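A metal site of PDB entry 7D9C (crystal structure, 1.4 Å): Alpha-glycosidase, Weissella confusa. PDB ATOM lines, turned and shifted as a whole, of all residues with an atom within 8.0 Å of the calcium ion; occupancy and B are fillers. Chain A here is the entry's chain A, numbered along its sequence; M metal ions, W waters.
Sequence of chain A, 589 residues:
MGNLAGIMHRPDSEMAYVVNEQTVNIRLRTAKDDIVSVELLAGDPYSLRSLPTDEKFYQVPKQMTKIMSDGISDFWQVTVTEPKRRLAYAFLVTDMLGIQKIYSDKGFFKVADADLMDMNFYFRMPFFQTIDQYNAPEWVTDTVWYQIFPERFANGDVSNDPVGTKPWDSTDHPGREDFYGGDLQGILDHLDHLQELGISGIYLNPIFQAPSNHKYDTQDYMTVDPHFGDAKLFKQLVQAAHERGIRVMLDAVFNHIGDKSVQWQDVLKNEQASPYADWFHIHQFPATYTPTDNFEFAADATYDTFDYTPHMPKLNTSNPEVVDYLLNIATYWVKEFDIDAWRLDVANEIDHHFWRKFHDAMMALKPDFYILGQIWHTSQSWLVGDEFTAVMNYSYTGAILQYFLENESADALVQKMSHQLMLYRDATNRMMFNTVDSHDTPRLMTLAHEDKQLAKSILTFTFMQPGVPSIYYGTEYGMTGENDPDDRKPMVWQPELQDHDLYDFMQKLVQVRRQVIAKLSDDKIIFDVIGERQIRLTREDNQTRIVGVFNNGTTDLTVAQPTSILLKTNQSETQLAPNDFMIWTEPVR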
ATOM      1  N   PRO A 150      -8.668  -8.383 -10.797  1.00  0.00           N
ATOM      2  CA  PRO A 150      -7.582  -8.159 -11.790  1.00  0.00           C
ATOM      3  C   PRO A 150      -6.214  -8.704 -11.386  1.00  0.00           C
ATOM      4  O   PRO A 150      -5.433  -9.102 -12.258  1.00  0.00           O
ATOM      5  CB  PRO A 150      -7.575  -6.654 -12.035  1.00  0.00           C
ATOM      6  CG  PRO A 150      -8.453  -6.080 -10.802  1.00  0.00           C
ATOM      7  CD  PRO A 150      -9.398  -7.156 -10.444  1.00  0.00           C
ATOM      8  N   GLU A 151      -5.906  -8.777 -10.092  1.00  0.00           N
ATOM      9  CA  GLU A 151      -4.597  -9.300  -9.696  1.00  0.00           C
ATOM     10  C   GLU A 151      -4.416 -10.758 -10.106  1.00  0.00           C
ATOM     11  O   GLU A 151      -3.265 -11.251 -10.186  1.00  0.00           O
ATOM     12  CB  GLU A 151      -4.431  -9.176  -8.176  1.00  0.00           C
ATOM     13  CG  GLU A 151      -3.024  -8.645  -7.752  1.00  0.00           C
ATOM     14  CD  GLU A 151      -1.889  -9.636  -7.833  1.00  0.00           C
ATOM     15  OE1 GLU A 151      -2.017 -10.777  -7.300  1.00  0.00           O
ATOM     16  OE2 GLU A 151      -0.814  -9.250  -8.382  1.00  0.00           O
ATOM     17  N   ALA A 154      -4.909 -12.330 -15.502  1.00  0.00           N
ATOM     18  CA  ALA A 154      -3.813 -12.652 -16.418  1.00  0.00           C
ATOM     19  C   ALA A 154      -2.699 -11.627 -16.249  1.00  0.00           C
ATOM     20  O   ALA A 154      -2.980 -10.429 -16.151  1.00  0.00           O
ATOM     21  CB  ALA A 154      -4.242 -12.714 -17.899  1.00  0.00           C
ATOM     22  N   ASN A 155      -1.454 -12.107 -16.203  1.00  0.00           N
ATOM     23  CA  ASN A 155      -0.293 -11.222 -16.190  1.00  0.00           C
ATOM     24  C   ASN A 155       0.123 -10.954 -17.623  1.00  0.00           C
ATOM     25  O   ASN A 155       0.745 -11.791 -18.261  1.00  0.00           O
ATOM     26  CB  ASN A 155       0.835 -11.839 -15.394  1.00  0.00           C
ATOM     27  CG  ASN A 155       1.992 -10.890 -15.141  1.00  0.00           C
ATOM     28  OD1 ASN A 155       1.978  -9.705 -15.512  1.00  0.00           O
ATOM     29  ND2 ASN A 155       3.027 -11.414 -14.446  1.00  0.00           N
ATOM     30  N   GLY A 156      -0.195  -9.781 -18.140  1.00  0.00           N
ATOM     31  CA  GLY A 156       0.256  -9.363 -19.447  1.00  0.00           C
ATOM     32  C   GLY A 156       1.522  -8.555 -19.455  1.00  0.00           C
ATOM     33  O   GLY A 156       1.933  -8.102 -20.522  1.00  0.00           O
ATOM     34  N   ASP A 157       2.124  -8.292 -18.286  1.00  0.00           N
ATOM     35  CA  ASP A 157       3.305  -7.448 -18.249  1.00  0.00           C
ATOM     36  C   ASP A 157       4.054  -7.764 -16.946  1.00  0.00           C
ATOM     37  O   ASP A 157       3.681  -7.313 -15.866  1.00  0.00           O
ATOM     38  CB  ASP A 157       2.874  -5.983 -18.325  1.00  0.00           C
ATOM     39  CG  ASP A 157       3.981  -5.020 -18.310  1.00  0.00           C
ATOM     40  OD1 ASP A 157       5.146  -5.440 -18.166  1.00  0.00           O
ATOM     41  OD2 ASP A 157       3.674  -3.810 -18.453  1.00  0.00           O
ATOM     42  N   VAL A 158       5.135  -8.540 -17.055  1.00  0.00           N
ATOM     43  CA  VAL A 158       5.924  -8.836 -15.844  1.00  0.00           C
ATOM     44  C   VAL A 158       6.607  -7.583 -15.316  1.00  0.00           C
ATOM     45  O   VAL A 158       6.931  -7.532 -14.128  1.00  0.00           O
ATOM     46  CB  VAL A 158       7.006  -9.918 -16.089  1.00  0.00           C
ATOM     47  CG1 VAL A 158       6.396 -11.254 -16.333  1.00  0.00           C
ATOM     48  CG2 VAL A 158       7.953  -9.511 -17.241  1.00  0.00           C
ATOM     49  N   SER A 159       6.811  -6.579 -16.149  1.00  0.00           N
ATOM     50  CA  SER A 159       7.597  -5.408 -15.732  1.00  0.00           C
ATOM     51  C   SER A 159       6.874  -4.521 -14.721  1.00  0.00           C
ATOM     52  O   SER A 159       7.539  -3.716 -14.079  1.00  0.00           O
ATOM     53  CB  SER A 159       8.074  -4.576 -16.945  1.00  0.00           C
ATOM     54  OG  SER A 159       7.026  -3.780 -17.452  1.00  0.00           O
ATOM     55  N   ASN A 160       5.564  -4.654 -14.559  1.00  0.00           N
ATOM     56  CA  ASN A 160       4.837  -3.891 -13.560  1.00  0.00           C
ATOM     57  C   ASN A 160       4.515  -4.713 -12.325  1.00  0.00           C
ATOM     58  O   ASN A 160       3.757  -4.249 -11.480  1.00  0.00           O
ATOM     59  CB  ASN A 160       3.585  -3.240 -14.148  1.00  0.00           C
ATOM     60  CG  ASN A 160       2.559  -4.282 -14.583  1.00  0.00           C
ATOM     61  OD1 ASN A 160       2.606  -5.455 -14.178  1.00  0.00           O
ATOM     62  ND2 ASN A 160       1.616  -3.838 -15.456  1.00  0.00           N
ATOM     63  N   ASP A 161       5.081  -5.907 -12.208  1.00  0.00           N
ATOM     64  CA  ASP A 161       4.691  -6.790 -11.120  1.00  0.00           C
ATOM     65  C   ASP A 161       5.155  -6.220  -9.784  1.00  0.00           C
ATOM     66  O   ASP A 161       6.259  -5.686  -9.687  1.00  0.00           O
ATOM     67  CB  ASP A 161       5.327  -8.162 -11.296  1.00  0.00           C
ATOM     68  CG  ASP A 161       4.655  -8.980 -12.412  1.00  0.00           C
ATOM     69  OD1 ASP A 161       3.633  -8.572 -12.981  1.00  0.00           O
ATOM     70  OD2 ASP A 161       5.236 -10.090 -12.730  1.00  0.00           O
ATOM     71  N   PRO A 162       4.349  -6.382  -8.730  1.00  0.00           N
ATOM     72  CA  PRO A 162       4.806  -6.045  -7.377  1.00  0.00           C
ATOM     73  C   PRO A 162       6.078  -6.791  -6.990  1.00  0.00           C
ATOM     74  O   PRO A 162       6.329  -7.914  -7.441  1.00  0.00           O
ATOM     75  CB  PRO A 162       3.611  -6.490  -6.498  1.00  0.00           C
ATOM     76  CG  PRO A 162       2.407  -6.354  -7.423  1.00  0.00           C
ATOM     77  CD  PRO A 162       2.957  -6.819  -8.769  1.00  0.00           C
ATOM     78  N   THR A 165       6.347 -11.010  -6.430  1.00  0.00           N
ATOM     79  CA  THR A 165       5.308 -11.700  -7.183  1.00  0.00           C
ATOM     80  C   THR A 165       5.696 -13.159  -7.365  1.00  0.00           C
ATOM     81  O   THR A 165       6.852 -13.493  -7.629  1.00  0.00           O
ATOM     82  CB  THR A 165       5.157 -10.987  -8.533  1.00  0.00           C
ATOM     83  OG1 THR A 165       4.533  -9.716  -8.334  1.00  0.00           O
ATOM     84  CG2 THR A 165       4.308 -11.792  -9.505  1.00  0.00           C
ATOM     85  N   TRP A 168       3.014 -17.834 -11.666  1.00  0.00           N
ATOM     86  CA  TRP A 168       1.586 -18.000 -11.915  1.00  0.00           C
ATOM     87  C   TRP A 168       1.225 -19.466 -11.770  1.00  0.00           C
ATOM     88  O   TRP A 168       1.739 -20.297 -12.500  1.00  0.00           O
ATOM     89  CB  TRP A 168       1.257 -17.550 -13.336  1.00  0.00           C
ATOM     90  CG  TRP A 168      -0.220 -17.339 -13.545  1.00  0.00           C
ATOM     91  CD1 TRP A 168      -1.185 -18.263 -13.880  1.00  0.00           C
ATOM     92  CD2 TRP A 168      -0.900 -16.078 -13.352  1.00  0.00           C
ATOM     93  NE1 TRP A 168      -2.416 -17.645 -13.952  1.00  0.00           N
ATOM     94  CE2 TRP A 168      -2.276 -16.308 -13.600  1.00  0.00           C
ATOM     95  CE3 TRP A 168      -0.494 -14.800 -12.974  1.00  0.00           C
ATOM     96  CZ2 TRP A 168      -3.235 -15.297 -13.543  1.00  0.00           C
ATOM     97  CZ3 TRP A 168      -1.434 -13.813 -12.845  1.00  0.00           C
ATOM     98  CH2 TRP A 168      -2.789 -14.048 -13.164  1.00  0.00           C
ATOM     99  N   TYR A 180       0.444 -12.123  -7.684  1.00  0.00           N
ATOM    100  CA  TYR A 180       0.733 -12.930  -8.865  1.00  0.00           C
ATOM    101  C   TYR A 180       0.942 -12.094 -10.124  1.00  0.00           C
ATOM    102  O   TYR A 180       1.318 -12.660 -11.168  1.00  0.00           O
ATOM    103  CB  TYR A 180      -0.357 -13.990  -9.051  1.00  0.00           C
ATOM    104  CG  TYR A 180      -0.290 -15.060  -8.029  1.00  0.00           C
ATOM    105  CD1 TYR A 180       0.482 -16.212  -8.225  1.00  0.00           C
ATOM    106  CD2 TYR A 180      -1.041 -14.976  -6.855  1.00  0.00           C
ATOM    107  CE1 TYR A 180       0.512 -17.216  -7.278  1.00  0.00           C
ATOM    108  CE2 TYR A 180      -1.006 -15.972  -5.882  1.00  0.00           C
ATOM    109  CZ  TYR A 180      -0.246 -17.106  -6.119  1.00  0.00           C
ATOM    110  OH  TYR A 180      -0.217 -18.095  -5.199  1.00  0.00           O
ATOM    111  N   GLY A 181       0.685 -10.780 -10.077  1.00  0.00           N
ATOM    112  CA  GLY A 181       1.064  -9.930 -11.190  1.00  0.00           C
ATOM    113  C   GLY A 181      -0.005  -9.711 -12.227  1.00  0.00           C
ATOM    114  O   GLY A 181       0.325  -9.114 -13.275  1.00  0.00           O
ATOM    115  N   GLY A 182      -1.236 -10.126 -11.967  1.00  0.00           N
ATOM    116  CA  GLY A 182      -2.327  -9.853 -12.925  1.00  0.00           C
ATOM    117  C   GLY A 182      -2.504  -8.363 -13.167  1.00  0.00           C
ATOM    118  O   GLY A 182      -2.357  -7.539 -12.260  1.00  0.00           O
ATOM    119  N   ASP A 183      -2.914  -7.988 -14.384  1.00  0.00           N
ATOM    120  CA  ASP A 183      -2.967  -6.566 -14.694  1.00  0.00           C
ATOM    121  C   ASP A 183      -3.896  -6.327 -15.884  1.00  0.00           C
ATOM    122  O   ASP A 183      -4.527  -7.253 -16.417  1.00  0.00           O
ATOM    123  CB  ASP A 183      -1.530  -6.055 -15.010  1.00  0.00           C
ATOM    124  CG  ASP A 183      -0.756  -6.923 -16.076  1.00  0.00           C
ATOM    125  OD1 ASP A 183      -1.439  -7.398 -17.013  1.00  0.00           O
ATOM    126  OD2 ASP A 183       0.480  -7.092 -15.871  1.00  0.00           O
ATOM    127  N   LEU A 184      -4.012  -5.062 -16.318  1.00  0.00           N
ATOM    128  CA  LEU A 184      -4.944  -4.740 -17.382  1.00  0.00           C
ATOM    129  C   LEU A 184      -4.494  -5.259 -18.717  1.00  0.00           C
ATOM    130  O   LEU A 184      -5.339  -5.631 -19.551  1.00  0.00           O
ATOM    131  CB  LEU A 184      -5.143  -3.212 -17.487  1.00  0.00           C
ATOM    132  CG  LEU A 184      -5.745  -2.462 -16.330  1.00  0.00           C
ATOM    133  CD1 LEU A 184      -5.918  -1.002 -16.701  1.00  0.00           C
ATOM    134  CD2 LEU A 184      -7.053  -3.101 -15.872  1.00  0.00           C
ATOM    135  N   GLN A 185      -3.173  -5.297 -18.979  1.00  0.00           N
ATOM    136  CA  GLN A 185      -2.737  -5.868 -20.248  1.00  0.00           C
ATOM    137  C   GLN A 185      -3.173  -7.320 -20.356  1.00  0.00           C
ATOM    138  O   GLN A 185      -3.537  -7.782 -21.424  1.00  0.00           O
ATOM    139  CB  GLN A 185      -1.211  -5.725 -20.395  1.00  0.00           C
ATOM    140  CG  GLN A 185      -0.726  -6.315 -21.745  1.00  0.00           C
ATOM    141  CD  GLN A 185      -1.209  -5.496 -22.915  1.00  0.00           C
ATOM    142  OE1 GLN A 185      -1.026  -4.290 -22.934  1.00  0.00           O
ATOM    143  NE2 GLN A 185      -1.796  -6.144 -23.908  1.00  0.00           N
ATOM    144  N   GLY A 186      -3.173  -8.039 -19.221  1.00  0.00           N
ATOM    145  CA  GLY A 186      -3.637  -9.428 -19.261  1.00  0.00           C
ATOM    146  C   GLY A 186      -5.099  -9.556 -19.637  1.00  0.00           C
ATOM    147  O   GLY A 186      -5.489 -10.493 -20.351  1.00  0.00           O
ATOM    148  N   PRO A 226      -0.462   1.573 -10.689  1.00  0.00           N
ATOM    149  CA  PRO A 226       0.636   1.355 -11.678  1.00  0.00           C
ATOM    150  C   PRO A 226       1.047  -0.106 -11.833  1.00  0.00           C
ATOM    151  O   PRO A 226       1.653  -0.457 -12.864  1.00  0.00           O
ATOM    152  CB  PRO A 226       1.779   2.204 -11.137  1.00  0.00           C
ATOM    153  CG  PRO A 226       1.412   2.479  -9.734  1.00  0.00           C
ATOM    154  CD  PRO A 226      -0.091   2.521  -9.638  1.00  0.00           C
ATOM    155  N   HIS A 227       0.687  -0.983 -10.899  1.00  0.00           N
ATOM    156  CA  HIS A 227       0.932  -2.418 -11.110  1.00  0.00           C
ATOM    157  C   HIS A 227      -0.103  -3.019 -12.038  1.00  0.00           C
ATOM    158  O   HIS A 227       0.114  -4.138 -12.528  1.00  0.00           O
ATOM    159  CB  HIS A 227       0.933  -3.185  -9.784  1.00  0.00           C
ATOM    160  CG  HIS A 227       1.946  -2.682  -8.819  1.00  0.00           C
ATOM    161  ND1 HIS A 227       1.632  -1.741  -7.859  1.00  0.00           N
ATOM    162  CD2 HIS A 227       3.285  -2.878  -8.728  1.00  0.00           C
ATOM    163  CE1 HIS A 227       2.729  -1.398  -7.189  1.00  0.00           C
ATOM    164  NE2 HIS A 227       3.744  -2.116  -7.674  1.00  0.00           N
ATOM    165  N   PHE A 228      -1.198  -2.318 -12.275  1.00  0.00           N
ATOM    166  CA  PHE A 228      -2.209  -2.733 -13.231  1.00  0.00           C
ATOM    167  C   PHE A 228      -2.039  -2.087 -14.587  1.00  0.00           C
ATOM    168  O   PHE A 228      -2.420  -2.692 -15.588  1.00  0.00           O
ATOM    169  CB  PHE A 228      -3.626  -2.466 -12.687  1.00  0.00           C
ATOM    170  CG  PHE A 228      -4.082  -3.405 -11.581  1.00  0.00           C
ATOM    171  CD1 PHE A 228      -3.432  -4.565 -11.213  1.00  0.00           C
ATOM    172  CD2 PHE A 228      -5.290  -3.087 -10.912  1.00  0.00           C
ATOM    173  CE1 PHE A 228      -3.938  -5.455 -10.234  1.00  0.00           C
ATOM    174  CE2 PHE A 228      -5.774  -3.946  -9.895  1.00  0.00           C
ATOM    175  CZ  PHE A 228      -5.108  -5.136  -9.566  1.00  0.00           C
ATOM    176  N   GLY A 229      -1.571  -0.848 -14.652  1.00  0.00           N
ATOM    177  CA  GLY A 229      -1.577  -0.156 -15.928  1.00  0.00           C
ATOM    178  C   GLY A 229      -1.573   1.350 -15.738  1.00  0.00           C
ATOM    179  O   GLY A 229      -1.119   1.849 -14.711  1.00  0.00           O
HETATM  180 CA    CA M   1       1.972  -7.690 -14.236  1.00  0.00          CA
HETATM  181  O   HOH W   1       1.231  -6.630 -12.181  1.00  0.00           O
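N of Gly 181 sits at hydrogen-bond distance from OE2 of Glu 151, at 2.7 Å.
OD1 of Asp 157 sits at hydrogen-bond distance from OG of Ser 159, 2.6 Å away.
The backbone NH (N) of Asp 183 lies within hydrogen-bond range of the backbone carbonyl oxygen (O) of Pro 150.
The side-chain carboxylate of Asp 183 lies within hydrogen-bond range of the backbone NH of Gly 186 (2.9 Å).
ND2 of Asn 160 sits close to O of His 227, 3.3 Å away.
The backbone NH (N) of Gln 185 lies close to the side-chain carboxylate (OD1) of Asp 183 (3.4 Å).
N of Asp 183 lies within hydrogen-bond range of O of Ala 154.
The side-chain carboxylate of Asp 183 lies within hydrogen-bond range of the backbone NH of Gly 156 (2.9 Å).
Within 4 Å of the calcium ion: Asn 155, Asp 157, Asn 160, Asp 161, Gly 181 and Asp 183.
The calcium ion is bound by OD1 of Asp 161, OD2 of Asp 183, OD1 of Asn 160, O of Gly 181, OD1 of Asn 155, O of Asp 157 and water W1.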
